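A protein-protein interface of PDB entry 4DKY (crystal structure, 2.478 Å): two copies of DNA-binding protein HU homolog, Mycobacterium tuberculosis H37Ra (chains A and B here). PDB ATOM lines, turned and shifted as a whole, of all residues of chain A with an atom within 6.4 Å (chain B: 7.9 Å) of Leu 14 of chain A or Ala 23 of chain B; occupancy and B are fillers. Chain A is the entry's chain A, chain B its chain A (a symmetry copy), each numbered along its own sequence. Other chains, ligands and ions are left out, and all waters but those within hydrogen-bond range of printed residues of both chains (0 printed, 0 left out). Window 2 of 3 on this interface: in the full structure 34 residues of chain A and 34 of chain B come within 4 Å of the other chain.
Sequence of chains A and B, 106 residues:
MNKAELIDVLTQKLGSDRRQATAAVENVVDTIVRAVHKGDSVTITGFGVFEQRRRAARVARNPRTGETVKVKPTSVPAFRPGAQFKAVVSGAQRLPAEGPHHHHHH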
ATOM      1  N   VAL A   9     -39.000   0.072 -30.621  1.00  0.00           N
ATOM      2  CA  VAL A   9     -38.362  -1.232 -31.024  1.00  0.00           C
ATOM      3  C   VAL A   9     -37.354  -1.825 -30.097  1.00  0.00           C
ATOM      4  O   VAL A   9     -37.408  -2.991 -29.796  1.00  0.00           O
ATOM      5  CB  VAL A   9     -37.635  -1.103 -32.336  1.00  0.00           C
ATOM      6  CG1 VAL A   9     -37.080  -2.462 -32.659  1.00  0.00           C
ATOM      7  CG2 VAL A   9     -38.581  -0.681 -33.360  1.00  0.00           C
ATOM      8  N   LEU A  10     -36.405  -1.017 -29.695  1.00  0.00           N
ATOM      9  CA  LEU A  10     -35.404  -1.425 -28.768  1.00  0.00           C
ATOM     10  C   LEU A  10     -36.041  -1.793 -27.426  1.00  0.00           C
ATOM     11  O   LEU A  10     -35.528  -2.693 -26.705  1.00  0.00           O
ATOM     12  CB  LEU A  10     -34.453  -0.262 -28.552  1.00  0.00           C
ATOM     13  CG  LEU A  10     -33.169  -0.630 -27.802  1.00  0.00           C
ATOM     14  CD1 LEU A  10     -32.399  -1.775 -28.496  1.00  0.00           C
ATOM     15  CD2 LEU A  10     -32.260   0.579 -27.611  1.00  0.00           C
ATOM     16  N   THR A  11     -37.114  -1.140 -27.021  1.00  0.00           N
ATOM     17  CA  THR A  11     -37.753  -1.519 -25.754  1.00  0.00           C
ATOM     18  C   THR A  11     -38.250  -3.006 -25.797  1.00  0.00           C
ATOM     19  O   THR A  11     -37.950  -3.765 -24.909  1.00  0.00           O
ATOM     20  CB  THR A  11     -38.941  -0.561 -25.412  1.00  0.00           C
ATOM     21  OG1 THR A  11     -38.479   0.816 -25.353  1.00  0.00           O
ATOM     22  CG2 THR A  11     -39.608  -0.969 -24.067  1.00  0.00           C
ATOM     23  N   GLN A  12     -39.003  -3.389 -26.842  1.00  0.00           N
ATOM     24  CA  GLN A  12     -39.403  -4.769 -27.133  1.00  0.00           C
ATOM     25  C   GLN A  12     -38.222  -5.737 -27.267  1.00  0.00           C
ATOM     26  O   GLN A  12     -38.243  -6.928 -26.843  1.00  0.00           O
ATOM     27  CB  GLN A  12     -40.053  -4.848 -28.501  1.00  0.00           C
ATOM     28  CG  GLN A  12     -41.093  -3.875 -28.725  1.00  0.00           C
ATOM     29  CD  GLN A  12     -41.795  -3.642 -27.430  1.00  0.00           C
ATOM     30  OE1 GLN A  12     -41.424  -2.783 -26.638  1.00  0.00           O
ATOM     31  NE2 GLN A  12     -42.790  -4.452 -27.178  1.00  0.00           N
ATOM     32  N   LYS A  13     -37.187  -5.321 -27.919  1.00  0.00           N
ATOM     33  CA  LYS A  13     -36.171  -6.309 -28.004  1.00  0.00           C
ATOM     34  C   LYS A  13     -35.403  -6.443 -26.681  1.00  0.00           C
ATOM     35  O   LYS A  13     -34.749  -7.471 -26.385  1.00  0.00           O
ATOM     36  CB  LYS A  13     -35.270  -5.997 -29.147  1.00  0.00           C
ATOM     37  CG  LYS A  13     -35.889  -6.329 -30.449  1.00  0.00           C
ATOM     38  CD  LYS A  13     -35.086  -5.625 -31.501  1.00  0.00           C
ATOM     39  CE  LYS A  13     -35.375  -6.119 -32.892  1.00  0.00           C
ATOM     40  NZ  LYS A  13     -34.719  -5.171 -33.910  1.00  0.00           N
ATOM     41  N   LEU A  14     -35.419  -5.386 -25.887  1.00  0.00           N
ATOM     42  CA  LEU A  14     -34.548  -5.434 -24.687  1.00  0.00           C
ATOM     43  C   LEU A  14     -35.344  -6.083 -23.541  1.00  0.00           C
ATOM     44  O   LEU A  14     -34.788  -6.564 -22.575  1.00  0.00           O
ATOM     45  CB  LEU A  14     -34.091  -4.032 -24.259  1.00  0.00           C
ATOM     46  CG  LEU A  14     -32.868  -3.548 -24.989  1.00  0.00           C
ATOM     47  CD1 LEU A  14     -32.571  -2.222 -24.529  1.00  0.00           C
ATOM     48  CD2 LEU A  14     -31.720  -4.352 -24.580  1.00  0.00           C
ATOM     49  N   GLY A  15     -36.649  -6.097 -23.724  1.00  0.00           N
ATOM     50  CA  GLY A  15     -37.593  -6.325 -22.646  1.00  0.00           C
ATOM     51  C   GLY A  15     -37.244  -5.370 -21.487  1.00  0.00           C
ATOM     52  O   GLY A  15     -37.131  -5.787 -20.370  1.00  0.00           O
ATOM     53  N   SER A  16     -37.130  -4.089 -21.770  1.00  0.00           N
ATOM     54  CA  SER A  16     -36.746  -3.105 -20.804  1.00  0.00           C
ATOM     55  C   SER A  16     -37.970  -2.294 -20.524  1.00  0.00           C
ATOM     56  O   SER A  16     -38.983  -2.551 -21.119  1.00  0.00           O
ATOM     57  CB  SER A  16     -35.662  -2.233 -21.370  1.00  0.00           C
ATOM     58  OG  SER A  16     -36.131  -1.563 -22.496  1.00  0.00           O
ATOM     59  N   GLN A  20     -35.315   3.399 -19.939  1.00  0.00           N
ATOM     60  CA  GLN A  20     -34.122   2.578 -20.061  1.00  0.00           C
ATOM     61  C   GLN A  20     -33.572   2.417 -21.448  1.00  0.00           C
ATOM     62  O   GLN A  20     -32.408   2.493 -21.664  1.00  0.00           O
ATOM     63  CB  GLN A  20     -34.570   1.173 -19.726  1.00  0.00           C
ATOM     64  CG  GLN A  20     -34.029   0.535 -18.487  1.00  0.00           C
ATOM     65  CD  GLN A  20     -34.904  -0.614 -17.990  1.00  0.00           C
ATOM     66  OE1 GLN A  20     -35.967  -0.865 -18.500  1.00  0.00           O
ATOM     67  NE2 GLN A  20     -34.432  -1.311 -17.015  1.00  0.00           N
ATOM     68  N   ALA A  21     -34.474   2.175 -22.364  1.00  0.00           N
ATOM     69  CA  ALA A  21     -34.206   2.120 -23.747  1.00  0.00           C
ATOM     70  C   ALA A  21     -33.750   3.511 -24.203  1.00  0.00           C
ATOM     71  O   ALA A  21     -32.914   3.629 -25.025  1.00  0.00           O
ATOM     72  CB  ALA A  21     -35.428   1.631 -24.515  1.00  0.00           C
ATOM     73  N   ALA A  24     -30.355   4.308 -23.300  1.00  0.00           N
ATOM     74  CA  ALA A  24     -29.375   3.506 -24.062  1.00  0.00           C
ATOM     75  C   ALA A  24     -29.035   4.228 -25.319  1.00  0.00           C
ATOM     76  O   ALA A  24     -27.883   4.417 -25.671  1.00  0.00           O
ATOM     77  CB  ALA A  24     -29.908   2.085 -24.391  1.00  0.00           C
ATOM     78  N   ILE B   7     -18.828  -0.610 -24.893  1.00  0.00           N
ATOM     79  CA  ILE B   7     -19.825  -1.312 -24.100  1.00  0.00           C
ATOM     80  C   ILE B   7     -19.460  -1.049 -22.671  1.00  0.00           C
ATOM     81  O   ILE B   7     -20.320  -0.832 -21.864  1.00  0.00           O
ATOM     82  CB  ILE B   7     -19.908  -2.822 -24.395  1.00  0.00           C
ATOM     83  CG1 ILE B   7     -20.718  -3.028 -25.670  1.00  0.00           C
ATOM     84  CG2 ILE B   7     -20.692  -3.566 -23.240  1.00  0.00           C
ATOM     85  CD1 ILE B   7     -20.801  -4.479 -26.055  1.00  0.00           C
ATOM     86  N   LEU B  10     -20.847   2.531 -21.857  1.00  0.00           N
ATOM     87  CA  LEU B  10     -22.266   2.489 -21.749  1.00  0.00           C
ATOM     88  C   LEU B  10     -22.682   1.724 -20.490  1.00  0.00           C
ATOM     89  O   LEU B  10     -23.736   2.041 -19.873  1.00  0.00           O
ATOM     90  CB  LEU B  10     -22.814   1.760 -22.963  1.00  0.00           C
ATOM     91  CG  LEU B  10     -24.331   1.877 -23.136  1.00  0.00           C
ATOM     92  CD1 LEU B  10     -24.799   3.348 -23.190  1.00  0.00           C
ATOM     93  CD2 LEU B  10     -24.820   1.120 -24.366  1.00  0.00           C
ATOM     94  N   LEU B  14     -25.008   3.481 -17.815  1.00  0.00           N
ATOM     95  CA  LEU B  14     -26.399   2.970 -17.731  1.00  0.00           C
ATOM     96  C   LEU B  14     -26.650   2.493 -16.289  1.00  0.00           C
ATOM     97  O   LEU B  14     -27.774   2.362 -15.850  1.00  0.00           O
ATOM     98  CB  LEU B  14     -26.636   1.805 -18.702  1.00  0.00           C
ATOM     99  CG  LEU B  14     -27.001   2.244 -20.093  1.00  0.00           C
ATOM    100  CD1 LEU B  14     -27.156   1.072 -20.904  1.00  0.00           C
ATOM    101  CD2 LEU B  14     -28.325   2.858 -20.066  1.00  0.00           C
ATOM    102  N   ASP B  17     -25.816  -4.118 -15.937  1.00  0.00           N
ATOM    103  CA  ASP B  17     -24.720  -5.079 -16.002  1.00  0.00           C
ATOM    104  C   ASP B  17     -24.245  -5.066 -17.515  1.00  0.00           C
ATOM    105  O   ASP B  17     -24.902  -4.426 -18.367  1.00  0.00           O
ATOM    106  CB  ASP B  17     -25.080  -6.468 -15.435  1.00  0.00           C
ATOM    107  CG  ASP B  17     -26.208  -7.187 -16.233  1.00  0.00           C
ATOM    108  OD1 ASP B  17     -26.420  -6.906 -17.443  1.00  0.00           O
ATOM    109  OD2 ASP B  17     -26.915  -8.093 -15.666  1.00  0.00           O
ATOM    110  N   ARG B  18     -23.145  -5.759 -17.813  1.00  0.00           N
ATOM    111  CA  ARG B  18     -22.513  -5.664 -19.111  1.00  0.00           C
ATOM    112  C   ARG B  18     -23.335  -6.412 -20.141  1.00  0.00           C
ATOM    113  O   ARG B  18     -23.395  -6.065 -21.299  1.00  0.00           O
ATOM    114  CB  ARG B  18     -21.108  -6.228 -19.085  1.00  0.00           C
ATOM    115  CG  ARG B  18     -20.331  -6.096 -20.418  1.00  0.00           C
ATOM    116  CD  ARG B  18     -18.899  -6.716 -20.470  1.00  0.00           C
ATOM    117  NE  ARG B  18     -18.203  -6.374 -21.745  1.00  0.00           N
ATOM    118  CZ  ARG B  18     -17.473  -5.251 -21.945  1.00  0.00           C
ATOM    119  NH1 ARG B  18     -17.324  -4.378 -20.950  1.00  0.00           N
ATOM    120  NH2 ARG B  18     -16.864  -5.003 -23.104  1.00  0.00           N
ATOM    121  N   ARG B  19     -24.015  -7.463 -19.772  1.00  0.00           N
ATOM    122  CA  ARG B  19     -24.664  -8.238 -20.794  1.00  0.00           C
ATOM    123  C   ARG B  19     -25.715  -7.444 -21.521  1.00  0.00           C
ATOM    124  O   ARG B  19     -25.864  -7.546 -22.703  1.00  0.00           O
ATOM    125  CB  ARG B  19     -25.176  -9.542 -20.194  1.00  0.00           C
ATOM    126  CG  ARG B  19     -26.670  -9.748 -20.104  1.00  0.00           C
ATOM    127  CD  ARG B  19     -27.031 -11.225 -20.210  1.00  0.00           C
ATOM    128  NE  ARG B  19     -26.341 -11.878 -21.319  1.00  0.00           N
ATOM    129  CZ  ARG B  19     -25.349 -12.746 -21.166  1.00  0.00           C
ATOM    130  NH1 ARG B  19     -24.755 -13.265 -22.223  1.00  0.00           N
ATOM    131  NH2 ARG B  19     -24.948 -13.084 -19.948  1.00  0.00           N
ATOM    132  N   GLN B  20     -26.356  -6.642 -20.689  1.00  0.00           N
ATOM    133  CA  GLN B  20     -27.402  -5.662 -20.932  1.00  0.00           C
ATOM    134  C   GLN B  20     -27.031  -4.511 -21.819  1.00  0.00           C
ATOM    135  O   GLN B  20     -27.765  -4.123 -22.667  1.00  0.00           O
ATOM    136  CB  GLN B  20     -27.627  -4.984 -19.599  1.00  0.00           C
ATOM    137  CG  GLN B  20     -28.944  -5.181 -18.920  1.00  0.00           C
ATOM    138  CD  GLN B  20     -28.878  -4.902 -17.420  1.00  0.00           C
ATOM    139  OE1 GLN B  20     -27.831  -4.670 -16.867  1.00  0.00           O
ATOM    140  NE2 GLN B  20     -29.999  -4.905 -16.787  1.00  0.00           N
ATOM    141  N   ALA B  21     -25.862  -3.982 -21.562  1.00  0.00           N
ATOM    142  CA  ALA B  21     -25.253  -2.982 -22.348  1.00  0.00           C
ATOM    143  C   ALA B  21     -24.964  -3.572 -23.734  1.00  0.00           C
ATOM    144  O   ALA B  21     -25.076  -2.909 -24.703  1.00  0.00           O
ATOM    145  CB  ALA B  21     -23.995  -2.454 -21.670  1.00  0.00           C
ATOM    146  N   THR B  22     -24.580  -4.823 -23.780  1.00  0.00           N
ATOM    147  CA  THR B  22     -24.233  -5.534 -25.001  1.00  0.00           C
ATOM    148  C   THR B  22     -25.479  -5.760 -25.835  1.00  0.00           C
ATOM    149  O   THR B  22     -25.496  -5.531 -27.037  1.00  0.00           O
ATOM    150  CB  THR B  22     -23.608  -6.918 -24.674  1.00  0.00           C
ATOM    151  OG1 THR B  22     -22.258  -6.728 -24.179  1.00  0.00           O
ATOM    152  CG2 THR B  22     -23.551  -7.775 -25.952  1.00  0.00           C
ATOM    153  N   ALA B  23     -26.565  -6.168 -25.195  1.00  0.00           N
ATOM    154  CA  ALA B  23     -27.834  -6.278 -25.940  1.00  0.00           C
ATOM    155  C   ALA B  23     -28.216  -4.904 -26.533  1.00  0.00           C
ATOM    156  O   ALA B  23     -28.844  -4.794 -27.573  1.00  0.00           O
ATOM    157  CB  ALA B  23     -28.952  -6.803 -25.014  1.00  0.00           C
ATOM    158  N   ALA B  24     -27.870  -3.842 -25.845  1.00  0.00           N
ATOM    159  CA  ALA B  24     -28.367  -2.519 -26.278  1.00  0.00           C
ATOM    160  C   ALA B  24     -27.685  -2.141 -27.548  1.00  0.00           C
ATOM    161  O   ALA B  24     -28.299  -1.751 -28.526  1.00  0.00           O
ATOM    162  CB  ALA B  24     -28.136  -1.423 -25.202  1.00  0.00           C
ATOM    163  N   VAL B  25     -26.374  -2.234 -27.500  1.00  0.00           N
ATOM    164  CA  VAL B  25     -25.555  -1.858 -28.631  1.00  0.00           C
ATOM    165  C   VAL B  25     -25.807  -2.809 -29.814  1.00  0.00           C
ATOM    166  O   VAL B  25     -25.888  -2.382 -30.912  1.00  0.00           O
ATOM    167  CB  VAL B  25     -24.126  -1.995 -28.266  1.00  0.00           C
ATOM    168  CG1 VAL B  25     -23.335  -2.030 -29.598  1.00  0.00           C
ATOM    169  CG2 VAL B  25     -23.675  -0.869 -27.309  1.00  0.00           C
ATOM    170  N   GLU B  26     -25.902  -4.116 -29.599  1.00  0.00           N
ATOM    171  CA  GLU B  26     -26.230  -5.040 -30.678  1.00  0.00           C
ATOM    172  C   GLU B  26     -27.555  -4.830 -31.310  1.00  0.00           C
ATOM    173  O   GLU B  26     -27.759  -5.058 -32.507  1.00  0.00           O
ATOM    174  CB  GLU B  26     -26.091  -6.479 -30.185  1.00  0.00           C
ATOM    175  CG  GLU B  26     -24.615  -6.885 -30.345  1.00  0.00           C
ATOM    176  CD  GLU B  26     -24.262  -8.085 -29.602  1.00  0.00           C
ATOM    177  OE1 GLU B  26     -25.216  -8.744 -29.122  1.00  0.00           O
ATOM    178  OE2 GLU B  26     -23.026  -8.350 -29.451  1.00  0.00           O
ATOM    179  N   ASN B  27     -28.518  -4.391 -30.532  1.00  0.00           N
ATOM    180  CA  ASN B  27     -29.847  -4.324 -31.090  1.00  0.00           C
ATOM    181  C   ASN B  27     -30.191  -2.964 -31.619  1.00  0.00           C
ATOM    182  O   ASN B  27     -31.185  -2.865 -32.406  1.00  0.00           O
ATOM    183  CB  ASN B  27     -30.846  -4.647 -30.029  1.00  0.00           C
ATOM    184  CG  ASN B  27     -30.791  -6.079 -29.545  1.00  0.00           C
ATOM    185  OD1 ASN B  27     -31.158  -7.026 -30.227  1.00  0.00           O
ATOM    186  ND2 ASN B  27     -30.513  -6.193 -28.278  1.00  0.00           N
ATOM    187  N   VAL B  28     -29.503  -1.910 -31.135  1.00  0.00           N
ATOM    188  CA  VAL B  28     -29.527  -0.599 -31.868  1.00  0.00           C
ATOM    189  C   VAL B  28     -28.986  -0.729 -33.316  1.00  0.00           C
ATOM    190  O   VAL B  28     -29.646  -0.441 -34.293  1.00  0.00           O
ATOM    191  CB  VAL B  28     -28.663   0.439 -31.182  1.00  0.00           C
ATOM    192  CG1 VAL B  28     -28.416   1.545 -32.175  1.00  0.00           C
ATOM    193  CG2 VAL B  28     -29.448   1.060 -30.016  1.00  0.00           C
ATOM    194  N   VAL B  29     -27.749  -1.216 -33.394  1.00  0.00           N
ATOM    195  CA  VAL B  29     -27.091  -1.617 -34.612  1.00  0.00           C
ATOM    196  C   VAL B  29     -27.911  -2.478 -35.543  1.00  0.00           C
ATOM    197  O   VAL B  29     -28.255  -2.054 -36.658  1.00  0.00           O
ATOM    198  CB  VAL B  29     -25.846  -2.440 -34.261  1.00  0.00           C
ATOM    199  CG1 VAL B  29     -25.492  -3.234 -35.451  1.00  0.00           C
ATOM    200  CG2 VAL B  29     -24.682  -1.479 -33.789  1.00  0.00           C
ATOM    201  N   ASP B  30     -28.329  -3.614 -35.045  1.00  0.00           N
ATOM    202  CA  ASP B  30     -29.192  -4.514 -35.759  1.00  0.00           C
ATOM    203  C   ASP B  30     -30.421  -3.873 -36.250  1.00  0.00           C
ATOM    204  O   ASP B  30     -30.815  -4.112 -37.419  1.00  0.00           O
ATOM    205  CB  ASP B  30     -29.540  -5.695 -34.841  1.00  0.00           C
ATOM    206  CG  ASP B  30     -30.366  -6.744 -35.552  1.00  0.00           C
ATOM    207  OD1 ASP B  30     -31.032  -6.493 -36.588  1.00  0.00           O
ATOM    208  OD2 ASP B  30     -30.333  -7.884 -35.073  1.00  0.00           O
ATOM    209  N   THR B  31     -31.059  -3.058 -35.419  1.00  0.00           N
ATOM    210  CA  THR B  31     -32.326  -2.398 -35.864  1.00  0.00           C
ATOM    211  C   THR B  31     -32.072  -1.394 -37.024  1.00  0.00           C
ATOM    212  O   THR B  31     -32.841  -1.260 -37.969  1.00  0.00           O
ATOM    213  CB  THR B  31     -33.025  -1.657 -34.659  1.00  0.00           C
ATOM    214  OG1 THR B  31     -33.269  -2.605 -33.591  1.00  0.00           O
ATOM    215  CG2 THR B  31     -34.340  -0.881 -35.081  1.00  0.00           C
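NZ of Lys 13 of chain A is in hydrogen-bond range of OG1 of Thr 31 of chain B, 3.0 Å away.
The backbone carbonyl oxygen (O) of Asn 27 of chain B sits at hydrogen-bond distance from the side-chain hydroxyl (OG1) of Thr 31 of chain B, 2.4 Å away.
CG1 of Val 9 of chain A touches OG1 of Thr 31 of chain B (3.9 Å). Asn 27 of chain B touches Leu 10 of chain A. CG2 of Val 28 of chain B touches CD2 of Leu 10 of chain A, 3.7 Å away. CD2 of Leu 14 of chain A touches CB of Ala 23 of chain B, at 3.7 Å.
Of chain B, only Ala 23 (3.7 Å) comes within 4 Å of Leu 14 of chain A. Of chain A, only Leu 14 (3.7 Å) comes within 4 Å of Ala 23 of chain B. No residue of chain B comes within 4 Å of Gly 15 of chain A. Printed residues of chain A within 4 Å of Asn 27 of chain B: Leu 10 (3.6 Å). Of the printed residues of chain B, Leu 10 of chain A touches Asn 27 and Val 28. Of the printed residues of chain B, Lys 13 of chain A touches Thr 31 (3.0 Å). The nearest residue of chain B that does not touch Leu 14 of chain A is Ala 24 of chain B (4.1 Å). The nearest residue of chain A that does not touch Ala 23 of chain B is Leu 10 of chain A (4.8 Å). The nearest printed residue of chain A that does not touch Asn 27 of chain B is Leu 14 of chain A (4.3 Å).
Printed residues of chain A that touch a printed residue of chain B: Val 9, Leu 10, Lys 13 and Leu 14. Printed residues of chain B that touch a printed residue of chain A: Ala 23, Asn 27, Val 28 and Thr 31. Hydrophobic or aromatic side chains of chain B that line the printed part of chain A: Ala 23 and Val 28. Among the printed residues, no Asp or Glu carboxylate lies within 4 Å of a Lys or Arg side-chain nitrogen of the other chain.
5 positions are printed for both chains. Of the 5 pairs that touch across the chains among the printed residues, none has its exchanged pair printed and touching as well.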
